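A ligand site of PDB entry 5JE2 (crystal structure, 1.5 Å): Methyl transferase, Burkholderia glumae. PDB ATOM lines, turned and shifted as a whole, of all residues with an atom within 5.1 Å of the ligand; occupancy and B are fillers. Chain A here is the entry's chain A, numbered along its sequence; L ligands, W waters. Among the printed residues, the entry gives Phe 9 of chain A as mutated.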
ATOM      1  N   PHE A   9      -5.593 -18.589  27.430  1.00  0.00           N
ATOM      2  CA  PHE A   9      -6.924 -18.499  27.998  1.00  0.00           C
ATOM      3  C   PHE A   9      -7.668 -19.826  27.977  1.00  0.00           C
ATOM      4  O   PHE A   9      -8.743 -19.909  28.573  1.00  0.00           O
ATOM      5  CB  PHE A   9      -7.717 -17.379  27.287  1.00  0.00           C
ATOM      6  CG  PHE A   9      -7.442 -15.996  27.844  1.00  0.00           C
ATOM      7  CD1 PHE A   9      -8.419 -15.296  28.534  1.00  0.00           C
ATOM      8  CD2 PHE A   9      -6.186 -15.419  27.678  1.00  0.00           C
ATOM      9  CE1 PHE A   9      -8.150 -14.025  29.044  1.00  0.00           C
ATOM     10  CE2 PHE A   9      -5.908 -14.143  28.202  1.00  0.00           C
ATOM     11  CZ  PHE A   9      -6.905 -13.455  28.886  1.00  0.00           C
ATOM     12  N   PHE A  16     -12.439 -15.253  33.150  1.00  0.00           N
ATOM     13  CA  PHE A  16     -12.288 -13.915  32.599  1.00  0.00           C
ATOM     14  C   PHE A  16     -13.586 -13.129  32.751  1.00  0.00           C
ATOM     15  O   PHE A  16     -13.563 -11.967  33.187  1.00  0.00           O
ATOM     16  CB  PHE A  16     -11.832 -13.943  31.129  1.00  0.00           C
ATOM     17  CG  PHE A  16     -11.742 -12.575  30.546  1.00  0.00           C
ATOM     18  CD1 PHE A  16     -10.717 -11.713  30.929  1.00  0.00           C
ATOM     19  CD2 PHE A  16     -12.721 -12.106  29.685  1.00  0.00           C
ATOM     20  CE1 PHE A  16     -10.635 -10.423  30.430  1.00  0.00           C
ATOM     21  CE2 PHE A  16     -12.653 -10.790  29.198  1.00  0.00           C
ATOM     22  CZ  PHE A  16     -11.625  -9.959  29.576  1.00  0.00           C
ATOM     23  N   THR A  20     -14.471  -9.584  34.630  1.00  0.00           N
ATOM     24  CA  THR A  20     -15.142  -8.400  34.091  1.00  0.00           C
ATOM     25  C   THR A  20     -16.291  -7.953  34.984  1.00  0.00           C
ATOM     26  O   THR A  20     -16.666  -6.777  34.933  1.00  0.00           O
ATOM     27  CB  THR A  20     -15.676  -8.649  32.675  1.00  0.00           C
ATOM     28  OG1 THR A  20     -16.773  -9.594  32.698  1.00  0.00           O
ATOM     29  CG2 THR A  20     -14.582  -9.109  31.729  1.00  0.00           C
ATOM     30  N   ARG A  26     -13.059  -2.354  34.907  1.00  0.00           N
ATOM     31  CA  ARG A  26     -13.792  -2.800  33.711  1.00  0.00           C
ATOM     32  C   ARG A  26     -14.816  -1.774  33.251  1.00  0.00           C
ATOM     33  O   ARG A  26     -14.942  -1.521  32.049  1.00  0.00           O
ATOM     34  CB  ARG A  26     -14.464  -4.156  33.982  1.00  0.00           C
ATOM     35  CG  ARG A  26     -15.182  -4.735  32.761  1.00  0.00           C
ATOM     36  CD  ARG A  26     -14.267  -5.022  31.563  1.00  0.00           C
ATOM     37  NE  ARG A  26     -15.015  -5.764  30.561  1.00  0.00           N
ATOM     38  CZ  ARG A  26     -14.494  -6.329  29.468  1.00  0.00           C
ATOM     39  NH1 ARG A  26     -13.194  -6.219  29.184  1.00  0.00           N
ATOM     40  NH2 ARG A  26     -15.312  -7.022  28.659  1.00  0.00           N
ATOM     41  N   GLU A  29     -12.989   0.832  31.132  1.00  0.00           N
ATOM     42  CA  GLU A  29     -12.585   0.424  29.791  1.00  0.00           C
ATOM     43  C   GLU A  29     -13.799   0.237  28.886  1.00  0.00           C
ATOM     44  O   GLU A  29     -13.785   0.678  27.729  1.00  0.00           O
ATOM     45  CB  GLU A  29     -11.689  -0.822  29.829  1.00  0.00           C
ATOM     46  CG  GLU A  29     -12.297  -2.093  30.326  1.00  0.00           C
ATOM     47  CD  GLU A  29     -11.215  -3.117  30.688  1.00  0.00           C
ATOM     48  OE1 GLU A  29     -11.286  -4.265  30.190  1.00  0.00           O
ATOM     49  OE2 GLU A  29     -10.321  -2.790  31.499  1.00  0.00           O
ATOM     50  N   LEU A  48     -11.819  -8.580  17.379  1.00  0.00           N
ATOM     51  CA  LEU A  48     -10.607  -9.382  17.454  1.00  0.00           C
ATOM     52  C   LEU A  48     -10.176  -9.553  18.908  1.00  0.00           C
ATOM     53  O   LEU A  48     -10.377  -8.661  19.740  1.00  0.00           O
ATOM     54  CB  LEU A  48      -9.492  -8.732  16.646  1.00  0.00           C
ATOM     55  CG  LEU A  48      -9.745  -8.583  15.128  1.00  0.00           C
ATOM     56  CD1 LEU A  48      -8.549  -7.868  14.502  1.00  0.00           C
ATOM     57  CD2 LEU A  48      -9.975  -9.919  14.449  1.00  0.00           C
ATOM     58  N   ALA A  49      -9.590 -10.716  19.208  1.00  0.00           N
ATOM     59  CA  ALA A  49      -9.350 -11.139  20.595  1.00  0.00           C
ATOM     60  C   ALA A  49     -10.657 -11.057  21.384  1.00  0.00           C
ATOM     61  O   ALA A  49     -10.715 -10.482  22.471  1.00  0.00           O
ATOM     62  CB  ALA A  49      -8.256 -10.287  21.278  1.00  0.00           C
ATOM     63  N   CYS A  50     -11.715 -11.642  20.806  1.00  0.00           N
ATOM     64  CA  CYS A  50     -13.076 -11.383  21.281  1.00  0.00           C
ATOM     65  C   CYS A  50     -13.396 -12.018  22.622  1.00  0.00           C
ATOM     66  O   CYS A  50     -14.398 -11.612  23.215  1.00  0.00           O
ATOM     67  CB  CYS A  50     -14.101 -11.851  20.246  1.00  0.00           C
ATOM     68  SG  CYS A  50     -14.091 -13.621  19.900  1.00  0.00           S
ATOM     69  N   GLY A  51     -12.594 -12.964  23.108  1.00  0.00           N
ATOM     70  CA  GLY A  51     -12.931 -13.591  24.386  1.00  0.00           C
ATOM     71  C   GLY A  51     -14.241 -14.337  24.294  1.00  0.00           C
ATOM     72  O   GLY A  51     -14.476 -15.095  23.329  1.00  0.00           O
ATOM     73  N   PHE A  52     -15.110 -14.155  25.291  1.00  0.00           N
ATOM     74  CA  PHE A  52     -16.444 -14.764  25.213  1.00  0.00           C
ATOM     75  C   PHE A  52     -17.398 -13.941  24.356  1.00  0.00           C
ATOM     76  O   PHE A  52     -18.573 -14.304  24.240  1.00  0.00           O
ATOM     77  CB  PHE A  52     -17.048 -15.024  26.608  1.00  0.00           C
ATOM     78  CG  PHE A  52     -17.233 -13.793  27.447  1.00  0.00           C
ATOM     79  CD1 PHE A  52     -18.388 -13.044  27.358  1.00  0.00           C
ATOM     80  CD2 PHE A  52     -16.241 -13.389  28.335  1.00  0.00           C
ATOM     81  CE1 PHE A  52     -18.569 -11.902  28.128  1.00  0.00           C
ATOM     82  CE2 PHE A  52     -16.393 -12.236  29.112  1.00  0.00           C
ATOM     83  CZ  PHE A  52     -17.567 -11.488  28.999  1.00  0.00           C
ATOM     84  N   PHE A  54     -17.869 -10.349  24.432  1.00  0.00           N
ATOM     85  CA  PHE A  54     -18.572  -9.230  25.065  1.00  0.00           C
ATOM     86  C   PHE A  54     -18.786  -8.063  24.111  1.00  0.00           C
ATOM     87  O   PHE A  54     -19.913  -7.567  23.970  1.00  0.00           O
ATOM     88  CB  PHE A  54     -17.828  -8.725  26.304  1.00  0.00           C
ATOM     89  CG  PHE A  54     -18.545  -7.563  26.936  1.00  0.00           C
ATOM     90  CD1 PHE A  54     -19.654  -7.777  27.757  1.00  0.00           C
ATOM     91  CD2 PHE A  54     -18.140  -6.256  26.667  1.00  0.00           C
ATOM     92  CE1 PHE A  54     -20.344  -6.719  28.313  1.00  0.00           C
ATOM     93  CE2 PHE A  54     -18.829  -5.185  27.197  1.00  0.00           C
ATOM     94  CZ  PHE A  54     -19.929  -5.407  28.036  1.00  0.00           C
ATOM     95  N   PHE A  55     -17.712  -7.554  23.499  1.00  0.00           N
ATOM     96  CA  PHE A  55     -17.872  -6.303  22.771  1.00  0.00           C
ATOM     97  C   PHE A  55     -18.650  -6.515  21.481  1.00  0.00           C
ATOM     98  O   PHE A  55     -19.569  -5.763  21.185  1.00  0.00           O
ATOM     99  CB  PHE A  55     -16.507  -5.653  22.533  1.00  0.00           C
ATOM    100  CG  PHE A  55     -15.967  -5.024  23.764  1.00  0.00           C
ATOM    101  CD1 PHE A  55     -16.505  -3.810  24.236  1.00  0.00           C
ATOM    102  CD2 PHE A  55     -14.973  -5.666  24.525  1.00  0.00           C
ATOM    103  CE1 PHE A  55     -16.046  -3.234  25.415  1.00  0.00           C
ATOM    104  CE2 PHE A  55     -14.514  -5.089  25.704  1.00  0.00           C
ATOM    105  CZ  PHE A  55     -15.041  -3.875  26.154  1.00  0.00           C
ATOM    106  N   VAL A  70     -13.134 -13.210  16.551  1.00  0.00           N
ATOM    107  CA  VAL A  70     -11.939 -14.037  16.364  1.00  0.00           C
ATOM    108  C   VAL A  70     -11.166 -14.096  17.671  1.00  0.00           C
ATOM    109  O   VAL A  70     -10.932 -13.064  18.304  1.00  0.00           O
ATOM    110  CB  VAL A  70     -11.022 -13.493  15.248  1.00  0.00           C
ATOM    111  CG1 VAL A  70      -9.809 -14.404  15.052  1.00  0.00           C
ATOM    112  CG2 VAL A  70     -11.792 -13.371  13.929  1.00  0.00           C
ATOM    113  N   ASP A  71     -10.743 -15.303  18.057  1.00  0.00           N
ATOM    114  CA  ASP A  71      -9.900 -15.462  19.246  1.00  0.00           C
ATOM    115  C   ASP A  71      -8.971 -16.639  19.028  1.00  0.00           C
ATOM    116  O   ASP A  71      -9.338 -17.598  18.329  1.00  0.00           O
ATOM    117  CB  ASP A  71     -10.757 -15.696  20.502  1.00  0.00           C
ATOM    118  CG  ASP A  71     -10.008 -15.379  21.778  1.00  0.00           C
ATOM    119  OD1 ASP A  71     -10.230 -14.289  22.351  1.00  0.00           O
ATOM    120  OD2 ASP A  71      -9.223 -16.241  22.250  1.00  0.00           O
ATOM    121  N   ILE A  72      -7.783 -16.586  19.637  1.00  0.00           N
ATOM    122  CA  ILE A  72      -6.828 -17.698  19.520  1.00  0.00           C
ATOM    123  C   ILE A  72      -7.216 -18.906  20.371  1.00  0.00           C
ATOM    124  O   ILE A  72      -6.734 -20.024  20.117  1.00  0.00           O
ATOM    125  CB  ILE A  72      -5.415 -17.180  19.881  1.00  0.00           C
ATOM    126  CG1 ILE A  72      -4.325 -18.112  19.343  1.00  0.00           C
ATOM    127  CG2 ILE A  72      -5.301 -16.943  21.405  1.00  0.00           C
ATOM    128  CD1 ILE A  72      -2.935 -17.527  19.523  1.00  0.00           C
ATOM    129  N   SER A  73      -8.067 -18.719  21.384  1.00  0.00           N
ATOM    130  CA  SER A  73      -8.387 -19.782  22.345  1.00  0.00           C
ATOM    131  C   SER A  73      -9.640 -20.540  21.921  1.00  0.00           C
ATOM    132  O   SER A  73     -10.730 -19.969  21.865  1.00  0.00           O
ATOM    133  CB  SER A  73      -8.572 -19.177  23.738  1.00  0.00           C
ATOM    134  OG  SER A  73      -9.205 -20.082  24.639  1.00  0.00           O
ATOM    135  N   MET A  76     -12.200 -20.233  24.725  1.00  0.00           N
ATOM    136  CA  MET A  76     -12.940 -18.976  24.752  1.00  0.00           C
ATOM    137  C   MET A  76     -13.969 -18.923  23.628  1.00  0.00           C
ATOM    138  O   MET A  76     -15.063 -18.404  23.826  1.00  0.00           O
ATOM    139  CB  MET A  76     -11.993 -17.771  24.647  1.00  0.00           C
ATOM    140  CG  MET A  76     -11.009 -17.600  25.808  1.00  0.00           C
ATOM    141  SD  MET A  76     -11.744 -17.548  27.463  1.00  0.00           S
ATOM    142  CE  MET A  76     -12.472 -15.895  27.472  1.00  0.00           C
ATOM    143  N   ARG A  96      -8.486 -18.202  15.577  1.00  0.00           N
ATOM    144  CA  ARG A  96      -7.300 -17.810  14.828  1.00  0.00           C
ATOM    145  C   ARG A  96      -6.354 -17.061  15.737  1.00  0.00           C
ATOM    146  O   ARG A  96      -6.795 -16.337  16.633  1.00  0.00           O
ATOM    147  CB  ARG A  96      -7.586 -16.864  13.645  1.00  0.00           C
ATOM    148  CG  ARG A  96      -8.635 -17.299  12.627  1.00  0.00           C
ATOM    149  CD  ARG A  96      -8.080 -18.293  11.649  1.00  0.00           C
ATOM    150  NE  ARG A  96      -8.996 -18.471  10.520  1.00  0.00           N
ATOM    151  CZ  ARG A  96     -10.055 -19.277  10.526  1.00  0.00           C
ATOM    152  NH1 ARG A  96     -10.351 -19.975  11.622  1.00  0.00           N
ATOM    153  NH2 ARG A  96     -10.821 -19.369   9.446  1.00  0.00           N
ATOM    154  N   ASP A  97      -5.050 -17.184  15.445  1.00  0.00           N
ATOM    155  CA  ASP A  97      -4.039 -16.234  15.895  1.00  0.00           C
ATOM    156  C   ASP A  97      -4.096 -15.043  14.958  1.00  0.00           C
ATOM    157  O   ASP A  97      -3.784 -15.161  13.777  1.00  0.00           O
ATOM    158  CB  ASP A  97      -2.654 -16.892  15.891  1.00  0.00           C
ATOM    159  CG  ASP A  97      -1.529 -15.940  16.301  1.00  0.00           C
ATOM    160  OD1 ASP A  97      -1.783 -14.740  16.501  1.00  0.00           O
ATOM    161  OD2 ASP A  97      -0.370 -16.414  16.386  1.00  0.00           O
ATOM    162  N   VAL A  98      -4.492 -13.889  15.493  1.00  0.00           N
ATOM    163  CA  VAL A  98      -4.662 -12.727  14.627  1.00  0.00           C
ATOM    164  C   VAL A  98      -3.360 -12.329  13.941  1.00  0.00           C
ATOM    165  O   VAL A  98      -3.374 -11.842  12.818  1.00  0.00           O
ATOM    166  CB  VAL A  98      -5.272 -11.566  15.442  1.00  0.00           C
ATOM    167  CG1 VAL A  98      -5.184 -10.245  14.688  1.00  0.00           C
ATOM    168  CG2 VAL A  98      -6.715 -11.902  15.774  1.00  0.00           C
ATOM    169  N   ALA A  99      -2.196 -12.567  14.578  1.00  0.00           N
ATOM    170  CA  ALA A  99      -0.944 -12.197  13.932  1.00  0.00           C
ATOM    171  C   ALA A  99      -0.711 -12.954  12.630  1.00  0.00           C
ATOM    172  O   ALA A  99       0.002 -12.456  11.746  1.00  0.00           O
ATOM    173  CB  ALA A  99       0.244 -12.394  14.873  1.00  0.00           C
ATOM    174  N   ALA A 113     -10.207  -5.064  21.603  1.00  0.00           N
ATOM    175  CA  ALA A 113     -10.091  -4.776  23.030  1.00  0.00           C
ATOM    176  C   ALA A 113      -9.216  -5.851  23.653  1.00  0.00           C
ATOM    177  O   ALA A 113      -9.637  -7.005  23.798  1.00  0.00           O
ATOM    178  CB  ALA A 113     -11.466  -4.727  23.688  1.00  0.00           C
ATOM    179  N   TRP A 114      -7.978  -5.475  23.980  1.00  0.00           N
ATOM    180  CA  TRP A 114      -6.983  -6.394  24.552  1.00  0.00           C
ATOM    181  C   TRP A 114      -6.501  -7.436  23.537  1.00  0.00           C
ATOM    182  O   TRP A 114      -6.472  -8.650  23.808  1.00  0.00           O
ATOM    183  CB  TRP A 114      -7.516  -7.068  25.823  1.00  0.00           C
ATOM    184  CG  TRP A 114      -7.985  -6.075  26.870  1.00  0.00           C
ATOM    185  CD1 TRP A 114      -9.257  -5.896  27.327  1.00  0.00           C
ATOM    186  CD2 TRP A 114      -7.165  -5.120  27.567  1.00  0.00           C
ATOM    187  NE1 TRP A 114      -9.276  -4.897  28.286  1.00  0.00           N
ATOM    188  CE2 TRP A 114      -8.007  -4.395  28.442  1.00  0.00           C
ATOM    189  CE3 TRP A 114      -5.793  -4.794  27.521  1.00  0.00           C
ATOM    190  CZ2 TRP A 114      -7.515  -3.394  29.291  1.00  0.00           C
ATOM    191  CZ3 TRP A 114      -5.311  -3.798  28.378  1.00  0.00           C
ATOM    192  CH2 TRP A 114      -6.170  -3.111  29.256  1.00  0.00           C
ATOM    193  N   LEU A 115      -6.118  -6.944  22.358  1.00  0.00           N
ATOM    194  CA  LEU A 115      -5.429  -7.736  21.332  1.00  0.00           C
ATOM    195  C   LEU A 115      -3.931  -7.470  21.303  1.00  0.00           C
ATOM    196  O   LEU A 115      -3.135  -8.404  21.456  1.00  0.00           O
ATOM    197  CB  LEU A 115      -6.007  -7.446  19.935  1.00  0.00           C
ATOM    198  CG  LEU A 115      -5.193  -8.075  18.782  1.00  0.00           C
ATOM    199  CD1 LEU A 115      -5.281  -9.594  18.734  1.00  0.00           C
ATOM    200  CD2 LEU A 115      -5.658  -7.455  17.458  1.00  0.00           C
ATOM    201  N   TYR A 118      -1.073  -8.720  23.517  1.00  0.00           N
ATOM    202  CA  TYR A 118      -0.738 -10.138  23.476  1.00  0.00           C
ATOM    203  C   TYR A 118       0.179 -10.474  22.308  1.00  0.00           C
ATOM    204  O   TYR A 118       0.585 -11.637  22.186  1.00  0.00           O
ATOM    205  CB  TYR A 118      -2.012 -11.020  23.482  1.00  0.00           C
ATOM    206  CG  TYR A 118      -2.748 -10.887  24.785  1.00  0.00           C
ATOM    207  CD1 TYR A 118      -2.186 -11.352  25.966  1.00  0.00           C
ATOM    208  CD2 TYR A 118      -3.992 -10.275  24.848  1.00  0.00           C
ATOM    209  CE1 TYR A 118      -2.849 -11.198  27.203  1.00  0.00           C
ATOM    210  CE2 TYR A 118      -4.665 -10.122  26.084  1.00  0.00           C
ATOM    211  CZ  TYR A 118      -4.080 -10.593  27.240  1.00  0.00           C
ATOM    212  OH  TYR A 118      -4.731 -10.438  28.455  1.00  0.00           O
ATOM    213  N   MET A 128       0.093  -7.848  13.322  1.00  0.00           N
ATOM    214  CA  MET A 128      -1.303  -7.672  13.707  1.00  0.00           C
ATOM    215  C   MET A 128      -1.888  -6.403  13.113  1.00  0.00           C
ATOM    216  O   MET A 128      -3.021  -6.398  12.626  1.00  0.00           O
ATOM    217  CB  MET A 128      -1.461  -7.642  15.229  1.00  0.00           C
ATOM    218  CG  MET A 128      -1.289  -8.985  15.899  1.00  0.00           C
ATOM    219  SD  MET A 128      -1.661  -8.799  17.656  1.00  0.00           S
ATOM    220  CE  MET A 128      -1.440 -10.478  18.264  1.00  0.00           C
HETATM  221  N1  LIG L   1     -11.900  -8.573  24.056  1.00  0.00           N
HETATM  222  C1  LIG L   1     -12.562  -9.401  25.109  1.00  0.00           C
HETATM  223  C2  LIG L   1     -11.588 -10.429  25.691  1.00  0.00           C
HETATM  224  C3  LIG L   1     -10.299  -9.826  26.250  1.00  0.00           C
HETATM  225  S1  LIG L   1      -9.267 -11.076  27.034  1.00  0.00           S
HETATM  226  C4  LIG L   1     -13.065  -8.515  26.200  1.00  0.00           C
HETATM  227  O1  LIG L   1     -12.458  -7.478  26.551  1.00  0.00           O
HETATM  228  O2  LIG L   1     -14.124  -8.824  26.758  1.00  0.00           O
HETATM  229  C5  LIG L   1      -7.996 -11.278  25.809  1.00  0.00           C
HETATM  230  C6  LIG L   1      -8.356 -12.331  24.745  1.00  0.00           C
HETATM  231  O3  LIG L   1      -7.343 -12.223  23.732  1.00  0.00           O
HETATM  232  C7  LIG L   1      -8.320 -13.780  25.232  1.00  0.00           C
HETATM  233  O4  LIG L   1      -9.577 -14.432  24.976  1.00  0.00           O
HETATM  234  C8  LIG L   1      -7.180 -14.390  24.413  1.00  0.00           C
HETATM  235  O5  LIG L   1      -7.370 -15.780  24.068  1.00  0.00           O
HETATM  236  C9  LIG L   1      -7.153 -13.524  23.184  1.00  0.00           C
HETATM  237  N2  LIG L   1      -5.876 -13.541  22.439  1.00  0.00           N
HETATM  238  C10 LIG L   1      -4.628 -13.508  22.948  1.00  0.00           C
HETATM  239  N3  LIG L   1      -3.712 -13.545  21.947  1.00  0.00           N
HETATM  240  C11 LIG L   1      -4.386 -13.595  20.789  1.00  0.00           C
HETATM  241  C12 LIG L   1      -4.023 -13.647  19.384  1.00  0.00           C
HETATM  242  N4  LIG L   1      -2.715 -13.652  19.018  1.00  0.00           N
HETATM  243  N5  LIG L   1      -4.996 -13.702  18.464  1.00  0.00           N
HETATM  244  C13 LIG L   1      -6.303 -13.715  18.843  1.00  0.00           C
HETATM  245  N6  LIG L   1      -6.727 -13.659  20.113  1.00  0.00           N
HETATM  246  C14 LIG L   1      -5.811 -13.597  21.115  1.00  0.00           C
HETATM  247  O   HOH W   1      -7.192  -9.127  28.774  1.00  0.00           O
HETATM  248  O   HOH W   2     -12.112  -7.341  21.377  1.00  0.00           O
HETATM  249  O   HOH W   3      -3.230 -14.991  25.728  1.00  0.00           O
HETATM  250  O   HOH W   4     -15.520 -11.131  26.111  1.00  0.00           O
HETATM  251  O   HOH W   5     -15.055  -8.816  22.918  1.00  0.00           O
HETATM  252  O   HOH W   6      -1.649 -14.987  23.333  1.00  0.00           O
HETATM  253  O   HOH W   7      -0.250 -13.724  20.494  1.00  0.00           O
HETATM  254  O   HOH W   8      -5.124 -17.314  24.891  1.00  0.00           O
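OD2 of Asp 71 lies within hydrogen-bond range of O5 of the ligand, 2.6 Å away.
O of Ala 49 is in hydrogen-bond range of N1 of the ligand (2.7 Å).
O of Ala 113 is in hydrogen-bond range of N1 of the ligand, at 2.8 Å.
NH2 of Arg 26 lies within salt-bridge range of O2 of the ligand, 2.9 Å away.
N4 of the ligand is in hydrogen-bond range of OD1 of Asp 97 (2.9 Å).
N5 of the ligand is in hydrogen-bond range of N of Val 98 (3.0 Å).
The backbone NH (N) of Ile 72 is in hydrogen-bond range of a nitrogen (N6) of the ligand.
The side-chain carboxylate of Asp 71 lies within hydrogen-bond range of the backbone NH of Cys 50 (3.4 Å).
O of Asp 71 lies within hydrogen-bond range of N of Arg 96, 2.9 Å away.
The side-chain carboxylate (OD1) of Asp 71 sits at hydrogen-bond distance from the backbone NH (N) of Gly 51 (2.8 Å).
The backbone NH (N) of Ser 73 is in hydrogen-bond range of the side-chain carboxylate (OD2) of Asp 71, at 2.9 Å.
O of Val 70 sits at hydrogen-bond distance from N of Ala 49 (2.9 Å).
N of Ala 99 is in hydrogen-bond range of OD1 of Asp 97, at 2.9 Å.
O of Val 70 lies within hydrogen-bond range of N of Cys 50, 3.0 Å away.
N of Met 76 is in hydrogen-bond range of OG of Ser 73, 3.0 Å away.
Phe 9 touches the ligand.
CE2 of Phe 16 touches O2 of the ligand (3.5 Å).
O of Cys 50 touches C1 of the ligand, at 3.4 Å.
CA of Gly 51 touches O4 of the ligand, 3.5 Å away.
Phe 54 touches the ligand (CB to O2, 3.7 Å).
Phe 55 touches the ligand.
Ser 73 touches the ligand.
CG of Met 76 touches O4 of the ligand (3.6 Å).
O of Arg 96 touches C13 of the ligand, at 3.5 Å.
O of Trp 114 touches C5 of the ligand, 3.6 Å away.
Tyr 118 touches the ligand (CB to N3, 3.4 Å).
Met 128 touches the ligand.
Hydrophobic or aromatic side chains that line the ligand: Phe 9, Phe 16, Ala 49, Phe 54, Phe 55, Ile 72, Met 76, Val 98, Ala 113, Trp 114, Tyr 118 and Met 128.
19 residues have an atom within 4 Å of the ligand: Phe 9, Phe 16, Arg 26, Ala 49, Cys 50, Gly 51, Phe 54, Phe 55, Asp 71, Ile 72, Ser 73, Met 76, Arg 96, Asp 97, Val 98, Ala 113, Trp 114, Tyr 118 and Met 128.
The nearest printed residue that does not touch the ligand is Leu 115 (4.1 Å).
Water W4 lies within hydrogen-bond range of O2 of the ligand (2.8 Å), N of Phe 54 (3.0 Å), O of Cys 50 (3.1 Å) and N of Phe 52 (3.2 Å).
Water W8 bridges O5 of the ligand (2.8 Å) and N of Phe 9 (2.9 Å).
Water W7 bridges O of Tyr 118 (2.8 Å) and N4 of the ligand (2.9 Å).
Water W2 lies within hydrogen-bond range of the backbone carbonyl oxygen of Leu 48, a nitrogen (N1) of the ligand and the backbone NH of Ala 113.
Water W1 bridges the side-chain hydroxyl of Tyr 118 (2.8 Å) and a sulfur (S1) of the ligand (3.3 Å).
Water W5 lies within hydrogen-bond range of the backbone carbonyl oxygen (O) of Cys 50 (2.9 Å), the backbone NH (N) of Phe 55 (3.0 Å) and a nitrogen (N1) of the ligand (3.4 Å).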
